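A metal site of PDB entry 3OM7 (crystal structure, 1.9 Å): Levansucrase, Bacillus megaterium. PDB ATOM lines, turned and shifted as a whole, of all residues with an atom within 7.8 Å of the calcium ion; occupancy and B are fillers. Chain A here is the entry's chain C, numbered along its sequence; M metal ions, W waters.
The calcium ion is bound by water W1 (2.3 Å), O of Leu 290 (2.3 Å), OD1 of Asn 292 (2.3 Å), OD1 of Asp 223 (2.3 Å), OD1 of Asp 321 (2.4 Å), OE1 of Gln 254 (2.4 Å) and OD2 of Asp 321 (2.6 Å). The calcium ion has seven donor atoms within binding distance.
Within 4 Å of the calcium ion: Asp 223, Gln 254, Leu 290, Asn 292 and Asp 321.
Water W1 lies within hydrogen-bond range of OE1 of Gln 208, O of Asn 224 and ND2 of Asn 246.
The side-chain amide nitrogen of Asn 292 sits at hydrogen-bond distance from the side-chain hydroxyl of Thr 247 (2.8 Å). The side-chain carboxylate (OD2) of Asp 223 sits close to the side-chain carboxylate (OE2) of Glu 216 (2.6 Å). ND2 of Asn 246 lies within hydrogen-bond range of O of Asp 321 (3.0 Å). OE1 of Gln 254 sits close to NE2 of Gln 208, at 3.4 Å. NE2 of Gln 254 is in hydrogen-bond range of OE1 of Glu 216 (2.9 Å). The side-chain carboxylate (OD2) of Asp 321 lies close to the backbone NH (N) of Asn 224, 2.9 Å away. The side-chain carboxylate of Asp 223 is in hydrogen-bond range of the side-chain amide nitrogen of Gln 208 (3.3 Å).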
ATOM      1  N   GLN A 208       6.520 -12.736  28.969  1.00  0.00           N
ATOM      2  CA  GLN A 208       5.571 -13.441  29.826  1.00  0.00           C
ATOM      3  C   GLN A 208       5.869 -13.202  31.309  1.00  0.00           C
ATOM      4  O   GLN A 208       7.026 -13.146  31.709  1.00  0.00           O
ATOM      5  CB  GLN A 208       5.591 -14.941  29.508  1.00  0.00           C
ATOM      6  CG  GLN A 208       4.522 -15.758  30.227  1.00  0.00           C
ATOM      7  CD  GLN A 208       4.664 -17.247  29.968  1.00  0.00           C
ATOM      8  OE1 GLN A 208       5.707 -17.839  30.269  1.00  0.00           O
ATOM      9  NE2 GLN A 208       3.614 -17.853  29.426  1.00  0.00           N
ATOM     10  N   PHE A 213       1.553 -17.486  33.760  1.00  0.00           N
ATOM     11  CA  PHE A 213       1.852 -18.895  34.029  1.00  0.00           C
ATOM     12  C   PHE A 213       0.872 -19.493  35.040  1.00  0.00           C
ATOM     13  O   PHE A 213       0.359 -20.585  34.834  1.00  0.00           O
ATOM     14  CB  PHE A 213       3.315 -19.050  34.493  1.00  0.00           C
ATOM     15  CG  PHE A 213       3.701 -20.464  34.838  1.00  0.00           C
ATOM     16  CD1 PHE A 213       3.855 -21.426  33.848  1.00  0.00           C
ATOM     17  CD2 PHE A 213       3.935 -20.824  36.161  1.00  0.00           C
ATOM     18  CE1 PHE A 213       4.226 -22.731  34.162  1.00  0.00           C
ATOM     19  CE2 PHE A 213       4.311 -22.129  36.494  1.00  0.00           C
ATOM     20  CZ  PHE A 213       4.451 -23.083  35.496  1.00  0.00           C
ATOM     21  N   GLU A 216      -3.000 -19.741  33.621  1.00  0.00           N
ATOM     22  CA  GLU A 216      -3.233 -20.789  32.631  1.00  0.00           C
ATOM     23  C   GLU A 216      -3.346 -22.175  33.259  1.00  0.00           C
ATOM     24  O   GLU A 216      -3.831 -23.112  32.626  1.00  0.00           O
ATOM     25  CB  GLU A 216      -2.150 -20.771  31.541  1.00  0.00           C
ATOM     26  CG  GLU A 216      -0.832 -21.367  31.985  1.00  0.00           C
ATOM     27  CD  GLU A 216       0.287 -21.161  30.984  1.00  0.00           C
ATOM     28  OE1 GLU A 216       0.032 -21.240  29.761  1.00  0.00           O
ATOM     29  OE2 GLU A 216       1.423 -20.926  31.432  1.00  0.00           O
ATOM     30  N   GLY A 222       2.290 -28.021  31.359  1.00  0.00           N
ATOM     31  CA  GLY A 222       3.506 -28.335  30.622  1.00  0.00           C
ATOM     32  C   GLY A 222       4.195 -27.094  30.079  1.00  0.00           C
ATOM     33  O   GLY A 222       5.258 -27.190  29.443  1.00  0.00           O
ATOM     34  N   ASP A 223       3.600 -25.926  30.328  1.00  0.00           N
ATOM     35  CA  ASP A 223       4.252 -24.670  29.985  1.00  0.00           C
ATOM     36  C   ASP A 223       5.485 -24.468  30.864  1.00  0.00           C
ATOM     37  O   ASP A 223       5.526 -24.912  32.010  1.00  0.00           O
ATOM     38  CB  ASP A 223       3.286 -23.485  30.138  1.00  0.00           C
ATOM     39  CG  ASP A 223       3.775 -22.238  29.407  1.00  0.00           C
ATOM     40  OD1 ASP A 223       4.468 -22.358  28.371  1.00  0.00           O
ATOM     41  OD2 ASP A 223       3.466 -21.122  29.871  1.00  0.00           O
ATOM     42  N   ASN A 224       6.495 -23.801  30.303  1.00  0.00           N
ATOM     43  CA  ASN A 224       7.729 -23.528  31.037  1.00  0.00           C
ATOM     44  C   ASN A 224       8.027 -22.037  31.054  1.00  0.00           C
ATOM     45  O   ASN A 224       8.533 -21.478  30.069  1.00  0.00           O
ATOM     46  CB  ASN A 224       8.899 -24.325  30.447  1.00  0.00           C
ATOM     47  CG  ASN A 224      10.228 -24.066  31.175  1.00  0.00           C
ATOM     48  OD1 ASN A 224      10.259 -23.691  32.346  1.00  0.00           O
ATOM     49  ND2 ASN A 224      11.325 -24.268  30.456  1.00  0.00           N
ATOM     50  N   HIS A 225       7.705 -21.397  32.177  1.00  0.00           N
ATOM     51  CA  HIS A 225       7.931 -19.958  32.372  1.00  0.00           C
ATOM     52  C   HIS A 225       9.367 -19.682  32.805  1.00  0.00           C
ATOM     53  O   HIS A 225       9.863 -20.273  33.773  1.00  0.00           O
ATOM     54  CB  HIS A 225       6.965 -19.388  33.410  1.00  0.00           C
ATOM     55  CG  HIS A 225       7.227 -17.952  33.740  1.00  0.00           C
ATOM     56  ND1 HIS A 225       6.931 -16.921  32.863  1.00  0.00           N
ATOM     57  CD2 HIS A 225       7.763 -17.360  34.833  1.00  0.00           C
ATOM     58  CE1 HIS A 225       7.271 -15.765  33.413  1.00  0.00           C
ATOM     59  NE2 HIS A 225       7.782 -16.008  34.610  1.00  0.00           N
ATOM     60  N   THR A 226      10.027 -18.771  32.085  1.00  0.00           N
ATOM     61  CA  THR A 226      11.398 -18.375  32.384  1.00  0.00           C
ATOM     62  C   THR A 226      11.556 -16.847  32.353  1.00  0.00           C
ATOM     63  O   THR A 226      10.866 -16.156  31.599  1.00  0.00           O
ATOM     64  CB  THR A 226      12.426 -19.016  31.397  1.00  0.00           C
ATOM     65  OG1 THR A 226      12.385 -18.338  30.131  1.00  0.00           O
ATOM     66  CG2 THR A 226      12.153 -20.503  31.183  1.00  0.00           C
ATOM     67  N   ALA A 245      13.921 -15.386  28.491  1.00  0.00           N
ATOM     68  CA  ALA A 245      12.523 -15.125  28.805  1.00  0.00           C
ATOM     69  C   ALA A 245      11.608 -15.923  27.869  1.00  0.00           C
ATOM     70  O   ALA A 245      12.067 -16.812  27.146  1.00  0.00           O
ATOM     71  CB  ALA A 245      12.222 -13.625  28.716  1.00  0.00           C
ATOM     72  N   ASN A 246      10.309 -15.616  27.929  1.00  0.00           N
ATOM     73  CA  ASN A 246       9.351 -16.098  26.939  1.00  0.00           C
ATOM     74  C   ASN A 246       8.532 -14.910  26.446  1.00  0.00           C
ATOM     75  O   ASN A 246       8.384 -13.918  27.160  1.00  0.00           O
ATOM     76  CB  ASN A 246       8.435 -17.194  27.508  1.00  0.00           C
ATOM     77  CG  ASN A 246       9.220 -18.326  28.148  1.00  0.00           C
ATOM     78  OD1 ASN A 246       9.682 -18.223  29.282  1.00  0.00           O
ATOM     79  ND2 ASN A 246       9.391 -19.426  27.403  1.00  0.00           N
ATOM     80  N   THR A 247       8.019 -14.992  25.219  1.00  0.00           N
ATOM     81  CA  THR A 247       7.314 -13.866  24.616  1.00  0.00           C
ATOM     82  C   THR A 247       6.019 -13.566  25.357  1.00  0.00           C
ATOM     83  O   THR A 247       5.495 -14.413  26.091  1.00  0.00           O
ATOM     84  CB  THR A 247       6.957 -14.116  23.133  1.00  0.00           C
ATOM     85  OG1 THR A 247       6.172 -15.315  23.032  1.00  0.00           O
ATOM     86  CG2 THR A 247       8.202 -14.242  22.283  1.00  0.00           C
ATOM     87  N   TYR A 253       2.871 -14.708  20.860  1.00  0.00           N
ATOM     88  CA  TYR A 253       2.682 -15.516  22.050  1.00  0.00           C
ATOM     89  C   TYR A 253       2.562 -16.998  21.717  1.00  0.00           C
ATOM     90  O   TYR A 253       2.319 -17.379  20.564  1.00  0.00           O
ATOM     91  CB  TYR A 253       1.424 -15.057  22.800  1.00  0.00           C
ATOM     92  CG  TYR A 253       1.368 -15.426  24.267  1.00  0.00           C
ATOM     93  CD1 TYR A 253       2.499 -15.301  25.085  1.00  0.00           C
ATOM     94  CD2 TYR A 253       0.190 -15.867  24.850  1.00  0.00           C
ATOM     95  CE1 TYR A 253       2.445 -15.630  26.438  1.00  0.00           C
ATOM     96  CE2 TYR A 253       0.124 -16.197  26.195  1.00  0.00           C
ATOM     97  CZ  TYR A 253       1.250 -16.074  26.984  1.00  0.00           C
ATOM     98  OH  TYR A 253       1.162 -16.408  28.313  1.00  0.00           O
ATOM     99  N   GLN A 254       2.749 -17.835  22.739  1.00  0.00           N
ATOM    100  CA  GLN A 254       2.458 -19.254  22.657  1.00  0.00           C
ATOM    101  C   GLN A 254       0.965 -19.448  22.323  1.00  0.00           C
ATOM    102  O   GLN A 254       0.158 -18.519  22.436  1.00  0.00           O
ATOM    103  CB  GLN A 254       2.800 -19.941  23.982  1.00  0.00           C
ATOM    104  CG  GLN A 254       1.860 -19.579  25.135  1.00  0.00           C
ATOM    105  CD  GLN A 254       2.412 -19.936  26.502  1.00  0.00           C
ATOM    106  OE1 GLN A 254       3.619 -19.872  26.730  1.00  0.00           O
ATOM    107  NE2 GLN A 254       1.534 -20.325  27.416  1.00  0.00           N
ATOM    108  N   GLY A 255       0.616 -20.655  21.899  1.00  0.00           N
ATOM    109  CA  GLY A 255      -0.762 -20.992  21.559  1.00  0.00           C
ATOM    110  C   GLY A 255      -0.872 -21.655  20.199  1.00  0.00           C
ATOM    111  O   GLY A 255       0.093 -21.687  19.426  1.00  0.00           O
ATOM    112  N   LYS A 287       3.402 -29.419  22.647  1.00  0.00           N
ATOM    113  CA  LYS A 287       4.722 -28.950  23.074  1.00  0.00           C
ATOM    114  C   LYS A 287       5.157 -27.723  22.262  1.00  0.00           C
ATOM    115  O   LYS A 287       5.622 -26.739  22.825  1.00  0.00           O
ATOM    116  CB  LYS A 287       5.748 -30.085  22.959  1.00  0.00           C
ATOM    117  CG  LYS A 287       7.095 -29.833  23.663  1.00  0.00           C
ATOM    118  CD  LYS A 287       7.919 -31.113  23.661  1.00  0.00           C
ATOM    119  CE  LYS A 287       9.357 -30.897  24.106  1.00  0.00           C
ATOM    120  NZ  LYS A 287      10.122 -32.177  24.003  1.00  0.00           N
ATOM    121  N   ALA A 288       4.966 -27.791  20.946  1.00  0.00           N
ATOM    122  CA  ALA A 288       5.334 -26.698  20.039  1.00  0.00           C
ATOM    123  C   ALA A 288       4.464 -25.465  20.254  1.00  0.00           C
ATOM    124  O   ALA A 288       4.954 -24.337  20.198  1.00  0.00           O
ATOM    125  CB  ALA A 288       5.277 -27.160  18.591  1.00  0.00           C
ATOM    126  N   SER A 289       3.168 -25.684  20.516  1.00  0.00           N
ATOM    127  CA  SER A 289       2.223 -24.596  20.750  1.00  0.00           C
ATOM    128  C   SER A 289       2.624 -23.783  21.981  1.00  0.00           C
ATOM    129  O   SER A 289       2.491 -22.558  21.993  1.00  0.00           O
ATOM    130  CB  SER A 289       0.799 -25.142  20.913  1.00  0.00           C
ATOM    131  OG  SER A 289       0.421 -25.910  19.788  1.00  0.00           O
ATOM    132  N   LEU A 290       3.107 -24.477  23.006  1.00  0.00           N
ATOM    133  CA  LEU A 290       3.542 -23.841  24.258  1.00  0.00           C
ATOM    134  C   LEU A 290       4.929 -23.200  24.149  1.00  0.00           C
ATOM    135  O   LEU A 290       5.274 -22.306  24.930  1.00  0.00           O
ATOM    136  CB  LEU A 290       3.547 -24.860  25.411  1.00  0.00           C
ATOM    137  CG  LEU A 290       2.208 -25.338  25.984  1.00  0.00           C
ATOM    138  CD1 LEU A 290       2.394 -26.663  26.718  1.00  0.00           C
ATOM    139  CD2 LEU A 290       1.594 -24.293  26.902  1.00  0.00           C
ATOM    140  N   ALA A 291       5.713 -23.659  23.180  1.00  0.00           N
ATOM    141  CA  ALA A 291       7.089 -23.182  23.027  1.00  0.00           C
ATOM    142  C   ALA A 291       7.142 -21.745  22.510  1.00  0.00           C
ATOM    143  O   ALA A 291       6.801 -21.483  21.363  1.00  0.00           O
ATOM    144  CB  ALA A 291       7.883 -24.116  22.124  1.00  0.00           C
ATOM    145  N   ASN A 292       7.570 -20.827  23.377  1.00  0.00           N
ATOM    146  CA  ASN A 292       7.768 -19.425  22.998  1.00  0.00           C
ATOM    147  C   ASN A 292       8.960 -18.754  23.696  1.00  0.00           C
ATOM    148  O   ASN A 292       8.880 -17.589  24.107  1.00  0.00           O
ATOM    149  CB  ASN A 292       6.474 -18.610  23.213  1.00  0.00           C
ATOM    150  CG  ASN A 292       6.135 -18.398  24.690  1.00  0.00           C
ATOM    151  OD1 ASN A 292       6.297 -19.290  25.526  1.00  0.00           O
ATOM    152  ND2 ASN A 292       5.631 -17.214  24.994  1.00  0.00           N
ATOM    153  N   GLY A 293      10.072 -19.477  23.805  1.00  0.00           N
ATOM    154  CA  GLY A 293      11.308 -18.940  24.398  1.00  0.00           C
ATOM    155  C   GLY A 293      11.821 -17.710  23.673  1.00  0.00           C
ATOM    156  O   GLY A 293      11.625 -17.565  22.473  1.00  0.00           O
ATOM    157  N   THR A 320      11.355 -24.322  20.977  1.00  0.00           N
ATOM    158  CA  THR A 320      11.563 -24.605  22.393  1.00  0.00           C
ATOM    159  C   THR A 320      11.097 -23.474  23.302  1.00  0.00           C
ATOM    160  O   THR A 320      11.118 -22.305  22.922  1.00  0.00           O
ATOM    161  CB  THR A 320      13.041 -24.952  22.708  1.00  0.00           C
ATOM    162  OG1 THR A 320      13.179 -25.277  24.097  1.00  0.00           O
ATOM    163  CG2 THR A 320      13.968 -23.791  22.369  1.00  0.00           C
ATOM    164  N   ASP A 321      10.673 -23.845  24.509  1.00  0.00           N
ATOM    165  CA  ASP A 321      10.311 -22.888  25.538  1.00  0.00           C
ATOM    166  C   ASP A 321      11.553 -22.431  26.315  1.00  0.00           C
ATOM    167  O   ASP A 321      11.471 -21.498  27.111  1.00  0.00           O
ATOM    168  CB  ASP A 321       9.333 -23.548  26.499  1.00  0.00           C
ATOM    169  CG  ASP A 321       8.114 -22.689  26.770  1.00  0.00           C
ATOM    170  OD1 ASP A 321       7.995 -21.585  26.194  1.00  0.00           O
ATOM    171  OD2 ASP A 321       7.252 -23.136  27.551  1.00  0.00           O
ATOM    172  N   GLU A 322      12.694 -23.090  26.081  1.00  0.00           N
ATOM    173  CA  GLU A 322      13.863 -22.898  26.942  1.00  0.00           C
ATOM    174  C   GLU A 322      15.174 -22.638  26.189  1.00  0.00           C
ATOM    175  O   GLU A 322      15.907 -23.570  25.845  1.00  0.00           O
ATOM    176  CB  GLU A 322      13.995 -24.099  27.895  1.00  0.00           C
ATOM    177  CG  GLU A 322      15.019 -23.931  29.006  1.00  0.00           C
ATOM    178  CD  GLU A 322      14.921 -25.018  30.038  1.00  0.00           C
ATOM    179  OE1 GLU A 322      14.166 -24.848  31.012  1.00  0.00           O
ATOM    180  OE2 GLU A 322      15.602 -26.049  29.880  1.00  0.00           O
HETATM  181 CA    CA M   1       5.714 -21.098  26.842  1.00  0.00          CA
HETATM  182  O   HOH W   1       6.546 -19.965  28.636  1.00  0.00           O
